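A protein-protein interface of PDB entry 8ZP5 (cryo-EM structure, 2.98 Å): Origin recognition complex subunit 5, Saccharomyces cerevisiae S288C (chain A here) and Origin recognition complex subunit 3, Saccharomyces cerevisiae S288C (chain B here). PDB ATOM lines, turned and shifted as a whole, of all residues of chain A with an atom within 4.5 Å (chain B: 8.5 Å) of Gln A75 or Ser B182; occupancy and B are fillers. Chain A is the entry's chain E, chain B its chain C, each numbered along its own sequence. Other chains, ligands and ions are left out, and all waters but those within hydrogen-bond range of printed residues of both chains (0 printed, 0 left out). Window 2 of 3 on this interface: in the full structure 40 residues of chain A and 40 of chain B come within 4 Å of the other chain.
Hydrophobic or aromatic side chains of chain A within 4 Å of the printed part of chain B: Pro A72 and Leu A100.
The backbone NH of Ser B186 lies within hydrogen-bond range of the side-chain carboxylate of Asp B184.
OG of Ser B182 sits at hydrogen-bond distance from OD1 of Asp B184 (3.2 Å).
The side-chain amide nitrogen of Gln A75 sits close to the backbone carbonyl oxygen of Val A102, 3.3 Å away.
The backbone carbonyl oxygen (O) of Ser B186 sits at hydrogen-bond distance from the side-chain amide nitrogen (ND2) of Asn B190 (2.5 Å).
OE1 of Gln A75 sits at hydrogen-bond distance from OG of Ser B182 (3.3 Å).
Asp B184 touches Pro A72 (OD1 to CB, 3.3 Å).
OG of Ser B186 touches NH2 of Arg A79, at 3.8 Å.
Leu A100 touches Asp B180.
Printed residues of chain B within 4 Å of Pro A72: Asp B184.
Gln A75 touches one residue of chain B.
Of the printed residues of chain A, Ser B182 touches Gln A75.
Of the printed residues of chain A, Ser B186 touches Arg A79 (3.8 Å).
The nearest residue of chain B that does not touch Gln A75 is Asp B184 (5.7 Å).
The nearest printed residue of chain B that does not touch Arg A79 is Asn B190 (5.0 Å).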
ATOM      1  N   LYS A  71     -20.671   9.993 -20.381  1.00  0.00           N
ATOM      2  CA  LYS A  71     -19.968   9.092 -19.468  1.00  0.00           C
ATOM      3  C   LYS A  71     -18.933   8.228 -20.176  1.00  0.00           C
ATOM      4  O   LYS A  71     -17.804   8.113 -19.663  1.00  0.00           O
ATOM      5  CB  LYS A  71     -20.980   8.242 -18.694  1.00  0.00           C
ATOM      6  CG  LYS A  71     -21.322   8.782 -17.320  1.00  0.00           C
ATOM      7  CD  LYS A  71     -22.191   7.811 -16.542  1.00  0.00           C
ATOM      8  CE  LYS A  71     -21.413   6.573 -16.140  1.00  0.00           C
ATOM      9  NZ  LYS A  71     -22.183   5.734 -15.183  1.00  0.00           N
ATOM     10  N   PRO A  72     -19.230   7.582 -21.312  1.00  0.00           N
ATOM     11  CA  PRO A  72     -18.157   6.894 -22.043  1.00  0.00           C
ATOM     12  C   PRO A  72     -17.046   7.824 -22.481  1.00  0.00           C
ATOM     13  O   PRO A  72     -15.887   7.403 -22.517  1.00  0.00           O
ATOM     14  CB  PRO A  72     -18.889   6.284 -23.244  1.00  0.00           C
ATOM     15  CG  PRO A  72     -20.276   6.110 -22.777  1.00  0.00           C
ATOM     16  CD  PRO A  72     -20.544   7.303 -21.914  1.00  0.00           C
ATOM     17  N   LEU A  73     -17.360   9.080 -22.801  1.00  0.00           N
ATOM     18  CA  LEU A  73     -16.316  10.029 -23.179  1.00  0.00           C
ATOM     19  C   LEU A  73     -15.363  10.285 -22.018  1.00  0.00           C
ATOM     20  O   LEU A  73     -14.138  10.249 -22.184  1.00  0.00           O
ATOM     21  CB  LEU A  73     -16.951  11.335 -23.657  1.00  0.00           C
ATOM     22  CG  LEU A  73     -16.043  12.336 -24.369  1.00  0.00           C
ATOM     23  CD1 LEU A  73     -15.276  11.664 -25.490  1.00  0.00           C
ATOM     24  CD2 LEU A  73     -16.854  13.507 -24.898  1.00  0.00           C
ATOM     25  N   LEU A  74     -15.912  10.533 -20.826  1.00  0.00           N
ATOM     26  CA  LEU A  74     -15.069  10.760 -19.655  1.00  0.00           C
ATOM     27  C   LEU A  74     -14.251   9.522 -19.316  1.00  0.00           C
ATOM     28  O   LEU A  74     -13.054   9.621 -19.011  1.00  0.00           O
ATOM     29  CB  LEU A  74     -15.926  11.172 -18.460  1.00  0.00           C
ATOM     30  CG  LEU A  74     -16.933  12.306 -18.651  1.00  0.00           C
ATOM     31  CD1 LEU A  74     -17.851  12.396 -17.448  1.00  0.00           C
ATOM     32  CD2 LEU A  74     -16.229  13.627 -18.889  1.00  0.00           C
ATOM     33  N   GLN A  75     -14.879   8.345 -19.361  1.00  0.00           N
ATOM     34  CA  GLN A  75     -14.160   7.116 -19.039  1.00  0.00           C
ATOM     35  C   GLN A  75     -13.049   6.846 -20.046  1.00  0.00           C
ATOM     36  O   GLN A  75     -11.950   6.424 -19.668  1.00  0.00           O
ATOM     37  CB  GLN A  75     -15.134   5.942 -18.977  1.00  0.00           C
ATOM     38  CG  GLN A  75     -16.124   6.036 -17.832  1.00  0.00           C
ATOM     39  CD  GLN A  75     -17.261   5.050 -17.958  1.00  0.00           C
ATOM     40  OE1 GLN A  75     -17.268   4.204 -18.850  1.00  0.00           O
ATOM     41  NE2 GLN A  75     -18.235   5.154 -17.062  1.00  0.00           N
ATOM     42  N   ALA A  76     -13.312   7.090 -21.331  1.00  0.00           N
ATOM     43  CA  ALA A  76     -12.291   6.888 -22.351  1.00  0.00           C
ATOM     44  C   ALA A  76     -11.151   7.882 -22.198  1.00  0.00           C
ATOM     45  O   ALA A  76      -9.988   7.526 -22.405  1.00  0.00           O
ATOM     46  CB  ALA A  76     -12.910   6.991 -23.741  1.00  0.00           C
ATOM     47  N   ILE A  77     -11.458   9.132 -21.846  1.00  0.00           N
ATOM     48  CA  ILE A  77     -10.394  10.100 -21.589  1.00  0.00           C
ATOM     49  C   ILE A  77      -9.521   9.624 -20.436  1.00  0.00           C
ATOM     50  O   ILE A  77      -8.288   9.620 -20.527  1.00  0.00           O
ATOM     51  CB  ILE A  77     -10.983  11.493 -21.307  1.00  0.00           C
ATOM     52  CG1 ILE A  77     -11.560  12.102 -22.581  1.00  0.00           C
ATOM     53  CG2 ILE A  77      -9.923  12.411 -20.726  1.00  0.00           C
ATOM     54  CD1 ILE A  77     -12.284  13.398 -22.352  1.00  0.00           C
ATOM     55  N   ALA A  78     -10.153   9.194 -19.341  1.00  0.00           N
ATOM     56  CA  ALA A  78      -9.394   8.753 -18.175  1.00  0.00           C
ATOM     57  C   ALA A  78      -8.540   7.532 -18.494  1.00  0.00           C
ATOM     58  O   ALA A  78      -7.398   7.426 -18.031  1.00  0.00           O
ATOM     59  CB  ALA A  78     -10.340   8.458 -17.013  1.00  0.00           C
ATOM     60  N   ARG A  79      -9.078   6.594 -19.275  1.00  0.00           N
ATOM     61  CA  ARG A  79      -8.311   5.407 -19.645  1.00  0.00           C
ATOM     62  C   ARG A  79      -7.142   5.761 -20.556  1.00  0.00           C
ATOM     63  O   ARG A  79      -5.998   5.364 -20.301  1.00  0.00           O
ATOM     64  CB  ARG A  79      -9.227   4.389 -20.324  1.00  0.00           C
ATOM     65  CG  ARG A  79      -8.489   3.333 -21.128  1.00  0.00           C
ATOM     66  CD  ARG A  79      -9.447   2.304 -21.704  1.00  0.00           C
ATOM     67  NE  ARG A  79     -10.481   2.918 -22.528  1.00  0.00           N
ATOM     68  CZ  ARG A  79     -11.774   2.914 -22.235  1.00  0.00           C
ATOM     69  NH1 ARG A  79     -12.231   2.341 -21.134  1.00  0.00           N
ATOM     70  NH2 ARG A  79     -12.629   3.498 -23.068  1.00  0.00           N
ATOM     71  N   PRO A  99     -10.769   3.294 -15.105  1.00  0.00           N
ATOM     72  CA  PRO A  99     -11.527   4.336 -15.815  1.00  0.00           C
ATOM     73  C   PRO A  99     -13.024   4.266 -15.587  1.00  0.00           C
ATOM     74  O   PRO A  99     -13.704   5.288 -15.736  1.00  0.00           O
ATOM     75  CB  PRO A  99     -11.175   4.084 -17.287  1.00  0.00           C
ATOM     76  CG  PRO A  99     -10.739   2.658 -17.337  1.00  0.00           C
ATOM     77  CD  PRO A  99     -10.058   2.397 -16.031  1.00  0.00           C
ATOM     78  N   LEU A 100     -13.564   3.100 -15.232  1.00  0.00           N
ATOM     79  CA  LEU A 100     -15.000   2.977 -15.019  1.00  0.00           C
ATOM     80  C   LEU A 100     -15.467   3.655 -13.739  1.00  0.00           C
ATOM     81  O   LEU A 100     -16.678   3.804 -13.546  1.00  0.00           O
ATOM     82  CB  LEU A 100     -15.411   1.504 -15.005  1.00  0.00           C
ATOM     83  CG  LEU A 100     -15.742   0.888 -16.365  1.00  0.00           C
ATOM     84  CD1 LEU A 100     -14.476   0.520 -17.119  1.00  0.00           C
ATOM     85  CD2 LEU A 100     -16.641  -0.324 -16.199  1.00  0.00           C
ATOM     86  N   VAL A 102     -14.958   6.727 -13.227  1.00  0.00           N
ATOM     87  CA  VAL A 102     -15.255   8.093 -13.645  1.00  0.00           C
ATOM     88  C   VAL A 102     -16.707   8.141 -14.105  1.00  0.00           C
ATOM     89  O   VAL A 102     -17.040   7.658 -15.189  1.00  0.00           O
ATOM     90  CB  VAL A 102     -14.307   8.558 -14.754  1.00  0.00           C
ATOM     91  CG1 VAL A 102     -14.662   9.962 -15.188  1.00  0.00           C
ATOM     92  CG2 VAL A 102     -12.867   8.485 -14.284  1.00  0.00           C
ATOM     93  N   ARG B 140     -27.912   5.471 -28.909  1.00  0.00           N
ATOM     94  CA  ARG B 140     -27.167   5.079 -27.717  1.00  0.00           C
ATOM     95  C   ARG B 140     -27.632   3.725 -27.195  1.00  0.00           C
ATOM     96  O   ARG B 140     -26.809   2.886 -26.817  1.00  0.00           O
ATOM     97  CB  ARG B 140     -27.277   6.160 -26.637  1.00  0.00           C
ATOM     98  CG  ARG B 140     -28.597   6.236 -25.895  1.00  0.00           C
ATOM     99  CD  ARG B 140     -28.465   7.095 -24.649  1.00  0.00           C
ATOM    100  NE  ARG B 140     -27.279   6.752 -23.874  1.00  0.00           N
ATOM    101  CZ  ARG B 140     -27.271   5.916 -22.846  1.00  0.00           C
ATOM    102  NH1 ARG B 140     -28.375   5.313 -22.438  1.00  0.00           N
ATOM    103  NH2 ARG B 140     -26.130   5.681 -22.208  1.00  0.00           N
ATOM    104  N   LEU B 143     -26.467   0.889 -29.563  1.00  0.00           N
ATOM    105  CA  LEU B 143     -25.065   0.575 -29.312  1.00  0.00           C
ATOM    106  C   LEU B 143     -24.886  -0.171 -27.996  1.00  0.00           C
ATOM    107  O   LEU B 143     -24.123  -1.140 -27.926  1.00  0.00           O
ATOM    108  CB  LEU B 143     -24.225   1.850 -29.317  1.00  0.00           C
ATOM    109  CG  LEU B 143     -22.732   1.616 -29.096  1.00  0.00           C
ATOM    110  CD1 LEU B 143     -22.136   0.855 -30.268  1.00  0.00           C
ATOM    111  CD2 LEU B 143     -22.003   2.925 -28.883  1.00  0.00           C
ATOM    112  N   ARG B 144     -25.574   0.267 -26.937  1.00  0.00           N
ATOM    113  CA  ARG B 144     -25.412  -0.385 -25.643  1.00  0.00           C
ATOM    114  C   ARG B 144     -25.910  -1.824 -25.676  1.00  0.00           C
ATOM    115  O   ARG B 144     -25.248  -2.723 -25.148  1.00  0.00           O
ATOM    116  CB  ARG B 144     -26.126   0.414 -24.555  1.00  0.00           C
ATOM    117  CG  ARG B 144     -25.432   1.715 -24.202  1.00  0.00           C
ATOM    118  CD  ARG B 144     -26.096   2.402 -23.025  1.00  0.00           C
ATOM    119  NE  ARG B 144     -26.011   1.603 -21.810  1.00  0.00           N
ATOM    120  CZ  ARG B 144     -25.005   1.655 -20.947  1.00  0.00           C
ATOM    121  NH1 ARG B 144     -23.972   2.457 -21.140  1.00  0.00           N
ATOM    122  NH2 ARG B 144     -25.037   0.883 -19.866  1.00  0.00           N
ATOM    123  N   MET B 147     -23.391  -3.940 -27.779  1.00  0.00           N
ATOM    124  CA  MET B 147     -22.160  -4.242 -27.061  1.00  0.00           C
ATOM    125  C   MET B 147     -22.399  -5.168 -25.878  1.00  0.00           C
ATOM    126  O   MET B 147     -21.543  -6.003 -25.576  1.00  0.00           O
ATOM    127  CB  MET B 147     -21.477  -2.954 -26.605  1.00  0.00           C
ATOM    128  CG  MET B 147     -21.146  -2.006 -27.740  1.00  0.00           C
ATOM    129  SD  MET B 147     -20.041  -2.751 -28.950  1.00  0.00           S
ATOM    130  CE  MET B 147     -21.113  -2.839 -30.380  1.00  0.00           C
ATOM    131  N   TYR B 148     -23.541  -5.051 -25.198  1.00  0.00           N
ATOM    132  CA  TYR B 148     -23.838  -5.992 -24.124  1.00  0.00           C
ATOM    133  C   TYR B 148     -23.993  -7.405 -24.663  1.00  0.00           C
ATOM    134  O   TYR B 148     -23.459  -8.359 -24.084  1.00  0.00           O
ATOM    135  CB  TYR B 148     -25.097  -5.569 -23.370  1.00  0.00           C
ATOM    136  CG  TYR B 148     -25.537  -6.585 -22.343  1.00  0.00           C
ATOM    137  CD1 TYR B 148     -24.777  -6.824 -21.208  1.00  0.00           C
ATOM    138  CD2 TYR B 148     -26.705  -7.313 -22.513  1.00  0.00           C
ATOM    139  CE1 TYR B 148     -25.170  -7.755 -20.268  1.00  0.00           C
ATOM    140  CE2 TYR B 148     -27.106  -8.247 -21.577  1.00  0.00           C
ATOM    141  CZ  TYR B 148     -26.335  -8.463 -20.457  1.00  0.00           C
ATOM    142  OH  TYR B 148     -26.730  -9.391 -19.522  1.00  0.00           O
ATOM    143  N   LEU B 150     -22.671  -8.551 -27.440  1.00  0.00           N
ATOM    144  CA  LEU B 150     -21.355  -8.976 -27.904  1.00  0.00           C
ATOM    145  C   LEU B 150     -20.484  -9.438 -26.743  1.00  0.00           C
ATOM    146  O   LEU B 150     -19.845 -10.493 -26.815  1.00  0.00           O
ATOM    147  CB  LEU B 150     -20.684  -7.833 -28.666  1.00  0.00           C
ATOM    148  CG  LEU B 150     -19.168  -7.907 -28.827  1.00  0.00           C
ATOM    149  CD1 LEU B 150     -18.791  -9.085 -29.699  1.00  0.00           C
ATOM    150  CD2 LEU B 150     -18.630  -6.613 -29.409  1.00  0.00           C
ATOM    151  N   TYR B 151     -20.448  -8.659 -25.661  1.00  0.00           N
ATOM    152  CA  TYR B 151     -19.634  -9.026 -24.508  1.00  0.00           C
ATOM    153  C   TYR B 151     -20.141 -10.306 -23.859  1.00  0.00           C
ATOM    154  O   TYR B 151     -19.345 -11.173 -23.481  1.00  0.00           O
ATOM    155  CB  TYR B 151     -19.613  -7.882 -23.495  1.00  0.00           C
ATOM    156  CG  TYR B 151     -18.500  -7.989 -22.480  1.00  0.00           C
ATOM    157  CD1 TYR B 151     -17.238  -8.430 -22.849  1.00  0.00           C
ATOM    158  CD2 TYR B 151     -18.709  -7.646 -21.152  1.00  0.00           C
ATOM    159  CE1 TYR B 151     -16.217  -8.527 -21.925  1.00  0.00           C
ATOM    160  CE2 TYR B 151     -17.694  -7.741 -20.221  1.00  0.00           C
ATOM    161  CZ  TYR B 151     -16.450  -8.181 -20.613  1.00  0.00           C
ATOM    162  OH  TYR B 151     -15.435  -8.278 -19.691  1.00  0.00           O
ATOM    163  N   ASN B 179     -13.096  -8.780 -16.486  1.00  0.00           N
ATOM    164  CA  ASN B 179     -13.391  -7.695 -15.559  1.00  0.00           C
ATOM    165  C   ASN B 179     -14.657  -6.957 -15.981  1.00  0.00           C
ATOM    166  O   ASN B 179     -15.742  -7.538 -16.009  1.00  0.00           O
ATOM    167  CB  ASN B 179     -12.212  -6.725 -15.476  1.00  0.00           C
ATOM    168  CG  ASN B 179     -12.132  -6.017 -14.139  1.00  0.00           C
ATOM    169  OD1 ASN B 179     -12.940  -6.263 -13.244  1.00  0.00           O
ATOM    170  ND2 ASN B 179     -11.152  -5.133 -13.995  1.00  0.00           N
ATOM    171  N   ASP B 180     -14.516  -5.674 -16.307  1.00  0.00           N
ATOM    172  CA  ASP B 180     -15.635  -4.860 -16.756  1.00  0.00           C
ATOM    173  C   ASP B 180     -15.199  -4.002 -17.934  1.00  0.00           C
ATOM    174  O   ASP B 180     -14.041  -3.590 -18.028  1.00  0.00           O
ATOM    175  CB  ASP B 180     -16.176  -3.968 -15.633  1.00  0.00           C
ATOM    176  CG  ASP B 180     -17.231  -4.661 -14.798  1.00  0.00           C
ATOM    177  OD1 ASP B 180     -17.952  -5.523 -15.344  1.00  0.00           O
ATOM    178  OD2 ASP B 180     -17.342  -4.345 -13.595  1.00  0.00           O
ATOM    179  N   VAL B 181     -16.146  -3.738 -18.835  1.00  0.00           N
ATOM    180  CA  VAL B 181     -15.916  -2.897 -20.001  1.00  0.00           C
ATOM    181  C   VAL B 181     -17.086  -1.935 -20.144  1.00  0.00           C
ATOM    182  O   VAL B 181     -18.165  -2.141 -19.585  1.00  0.00           O
ATOM    183  CB  VAL B 181     -15.739  -3.715 -21.298  1.00  0.00           C
ATOM    184  CG1 VAL B 181     -14.535  -4.636 -21.195  1.00  0.00           C
ATOM    185  CG2 VAL B 181     -17.000  -4.505 -21.598  1.00  0.00           C
ATOM    186  N   SER B 182     -16.856  -0.869 -20.905  1.00  0.00           N
ATOM    187  CA  SER B 182     -17.905   0.086 -21.224  1.00  0.00           C
ATOM    188  C   SER B 182     -18.579  -0.318 -22.527  1.00  0.00           C
ATOM    189  O   SER B 182     -17.913  -0.681 -23.500  1.00  0.00           O
ATOM    190  CB  SER B 182     -17.338   1.502 -21.337  1.00  0.00           C
ATOM    191  OG  SER B 182     -18.377   2.455 -21.467  1.00  0.00           O
ATOM    192  N   TYR B 183     -19.910  -0.252 -22.540  1.00  0.00           N
ATOM    193  CA  TYR B 183     -20.704  -0.754 -23.660  1.00  0.00           C
ATOM    194  C   TYR B 183     -20.745   0.300 -24.761  1.00  0.00           C
ATOM    195  O   TYR B 183     -21.702   1.062 -24.915  1.00  0.00           O
ATOM    196  CB  TYR B 183     -22.099  -1.141 -23.191  1.00  0.00           C
ATOM    197  CG  TYR B 183     -22.103  -2.286 -22.207  1.00  0.00           C
ATOM    198  CD1 TYR B 183     -21.165  -3.303 -22.295  1.00  0.00           C
ATOM    199  CD2 TYR B 183     -23.039  -2.346 -21.186  1.00  0.00           C
ATOM    200  CE1 TYR B 183     -21.161  -4.350 -21.398  1.00  0.00           C
ATOM    201  CE2 TYR B 183     -23.044  -3.389 -20.285  1.00  0.00           C
ATOM    202  CZ  TYR B 183     -22.103  -4.388 -20.396  1.00  0.00           C
ATOM    203  OH  TYR B 183     -22.106  -5.428 -19.498  1.00  0.00           O
ATOM    204  N   ASP B 184     -19.670   0.338 -25.542  1.00  0.00           N
ATOM    205  CA  ASP B 184     -19.566   1.207 -26.707  1.00  0.00           C
ATOM    206  C   ASP B 184     -18.542   0.596 -27.660  1.00  0.00           C
ATOM    207  O   ASP B 184     -18.058  -0.519 -27.442  1.00  0.00           O
ATOM    208  CB  ASP B 184     -19.241   2.645 -26.279  1.00  0.00           C
ATOM    209  CG  ASP B 184     -17.930   2.759 -25.526  1.00  0.00           C
ATOM    210  OD1 ASP B 184     -17.921   3.382 -24.446  1.00  0.00           O
ATOM    211  OD2 ASP B 184     -16.906   2.246 -26.012  1.00  0.00           O
ATOM    212  N   LEU B 185     -18.208   1.328 -28.724  1.00  0.00           N
ATOM    213  CA  LEU B 185     -17.331   0.780 -29.754  1.00  0.00           C
ATOM    214  C   LEU B 185     -15.905   0.553 -29.272  1.00  0.00           C
ATOM    215  O   LEU B 185     -15.133  -0.109 -29.975  1.00  0.00           O
ATOM    216  CB  LEU B 185     -17.318   1.690 -30.982  1.00  0.00           C
ATOM    217  CG  LEU B 185     -18.405   1.438 -32.027  1.00  0.00           C
ATOM    218  CD1 LEU B 185     -18.240   2.383 -33.203  1.00  0.00           C
ATOM    219  CD2 LEU B 185     -18.379  -0.005 -32.493  1.00  0.00           C
ATOM    220  N   SER B 186     -15.528   1.084 -28.105  1.00  0.00           N
ATOM    221  CA  SER B 186     -14.217   0.758 -27.556  1.00  0.00           C
ATOM    222  C   SER B 186     -14.107  -0.727 -27.242  1.00  0.00           C
ATOM    223  O   SER B 186     -13.006  -1.286 -27.269  1.00  0.00           O
ATOM    224  CB  SER B 186     -13.937   1.591 -26.306  1.00  0.00           C
ATOM    225  OG  SER B 186     -13.970   2.975 -26.601  1.00  0.00           O
ATOM    226  N   LEU B 187     -15.233  -1.383 -26.954  1.00  0.00           N
ATOM    227  CA  LEU B 187     -15.219  -2.835 -26.811  1.00  0.00           C
ATOM    228  C   LEU B 187     -14.823  -3.508 -28.119  1.00  0.00           C
ATOM    229  O   LEU B 187     -14.027  -4.452 -28.124  1.00  0.00           O
ATOM    230  CB  LEU B 187     -16.584  -3.331 -26.339  1.00  0.00           C
ATOM    231  CG  LEU B 187     -16.786  -4.845 -26.259  1.00  0.00           C
ATOM    232  CD1 LEU B 187     -15.681  -5.500 -25.448  1.00  0.00           C
ATOM    233  CD2 LEU B 187     -18.146  -5.168 -25.668  1.00  0.00           C
ATOM    234  N   VAL B 188     -15.362  -3.029 -29.242  1.00  0.00           N
ATOM    235  CA  VAL B 188     -14.973  -3.574 -30.540  1.00  0.00           C
ATOM    236  C   VAL B 188     -13.505  -3.281 -30.817  1.00  0.00           C
ATOM    237  O   VAL B 188     -12.786  -4.109 -31.390  1.00  0.00           O
ATOM    238  CB  VAL B 188     -15.885  -3.012 -31.647  1.00  0.00           C
ATOM    239  CG1 VAL B 188     -15.417  -3.478 -33.015  1.00  0.00           C
ATOM    240  CG2 VAL B 188     -17.324  -3.427 -31.405  1.00  0.00           C
ATOM    241  N   ASN B 190     -11.060  -2.960 -28.580  1.00  0.00           N
ATOM    242  CA  ASN B 190     -10.208  -3.717 -27.675  1.00  0.00           C
ATOM    243  C   ASN B 190     -10.562  -5.198 -27.619  1.00  0.00           C
ATOM    244  O   ASN B 190     -10.060  -5.906 -26.742  1.00  0.00           O
ATOM    245  CB  ASN B 190     -10.278  -3.118 -26.269  1.00  0.00           C
ATOM    246  CG  ASN B 190     -10.104  -1.613 -26.267  1.00  0.00           C
ATOM    247  OD1 ASN B 190      -9.097  -1.092 -26.749  1.00  0.00           O
ATOM    248  ND2 ASN B 190     -11.086  -0.905 -25.723  1.00  0.00           N
ATOM    249  N   LEU B 194      -8.721  -8.167 -25.540  1.00  0.00           N
ATOM    250  CA  LEU B 194      -9.448  -8.807 -24.448  1.00  0.00           C
ATOM    251  C   LEU B 194      -9.539 -10.316 -24.641  1.00  0.00           C
ATOM    252  O   LEU B 194      -9.287 -11.085 -23.707  1.00  0.00           O
ATOM    253  CB  LEU B 194     -10.847  -8.200 -24.324  1.00  0.00           C
ATOM    254  CG  LEU B 194     -10.942  -6.806 -23.706  1.00  0.00           C
ATOM    255  CD1 LEU B 194     -12.348  -6.254 -23.856  1.00  0.00           C
ATOM    256  CD2 LEU B 194     -10.531  -6.841 -22.246  1.00  0.00           C
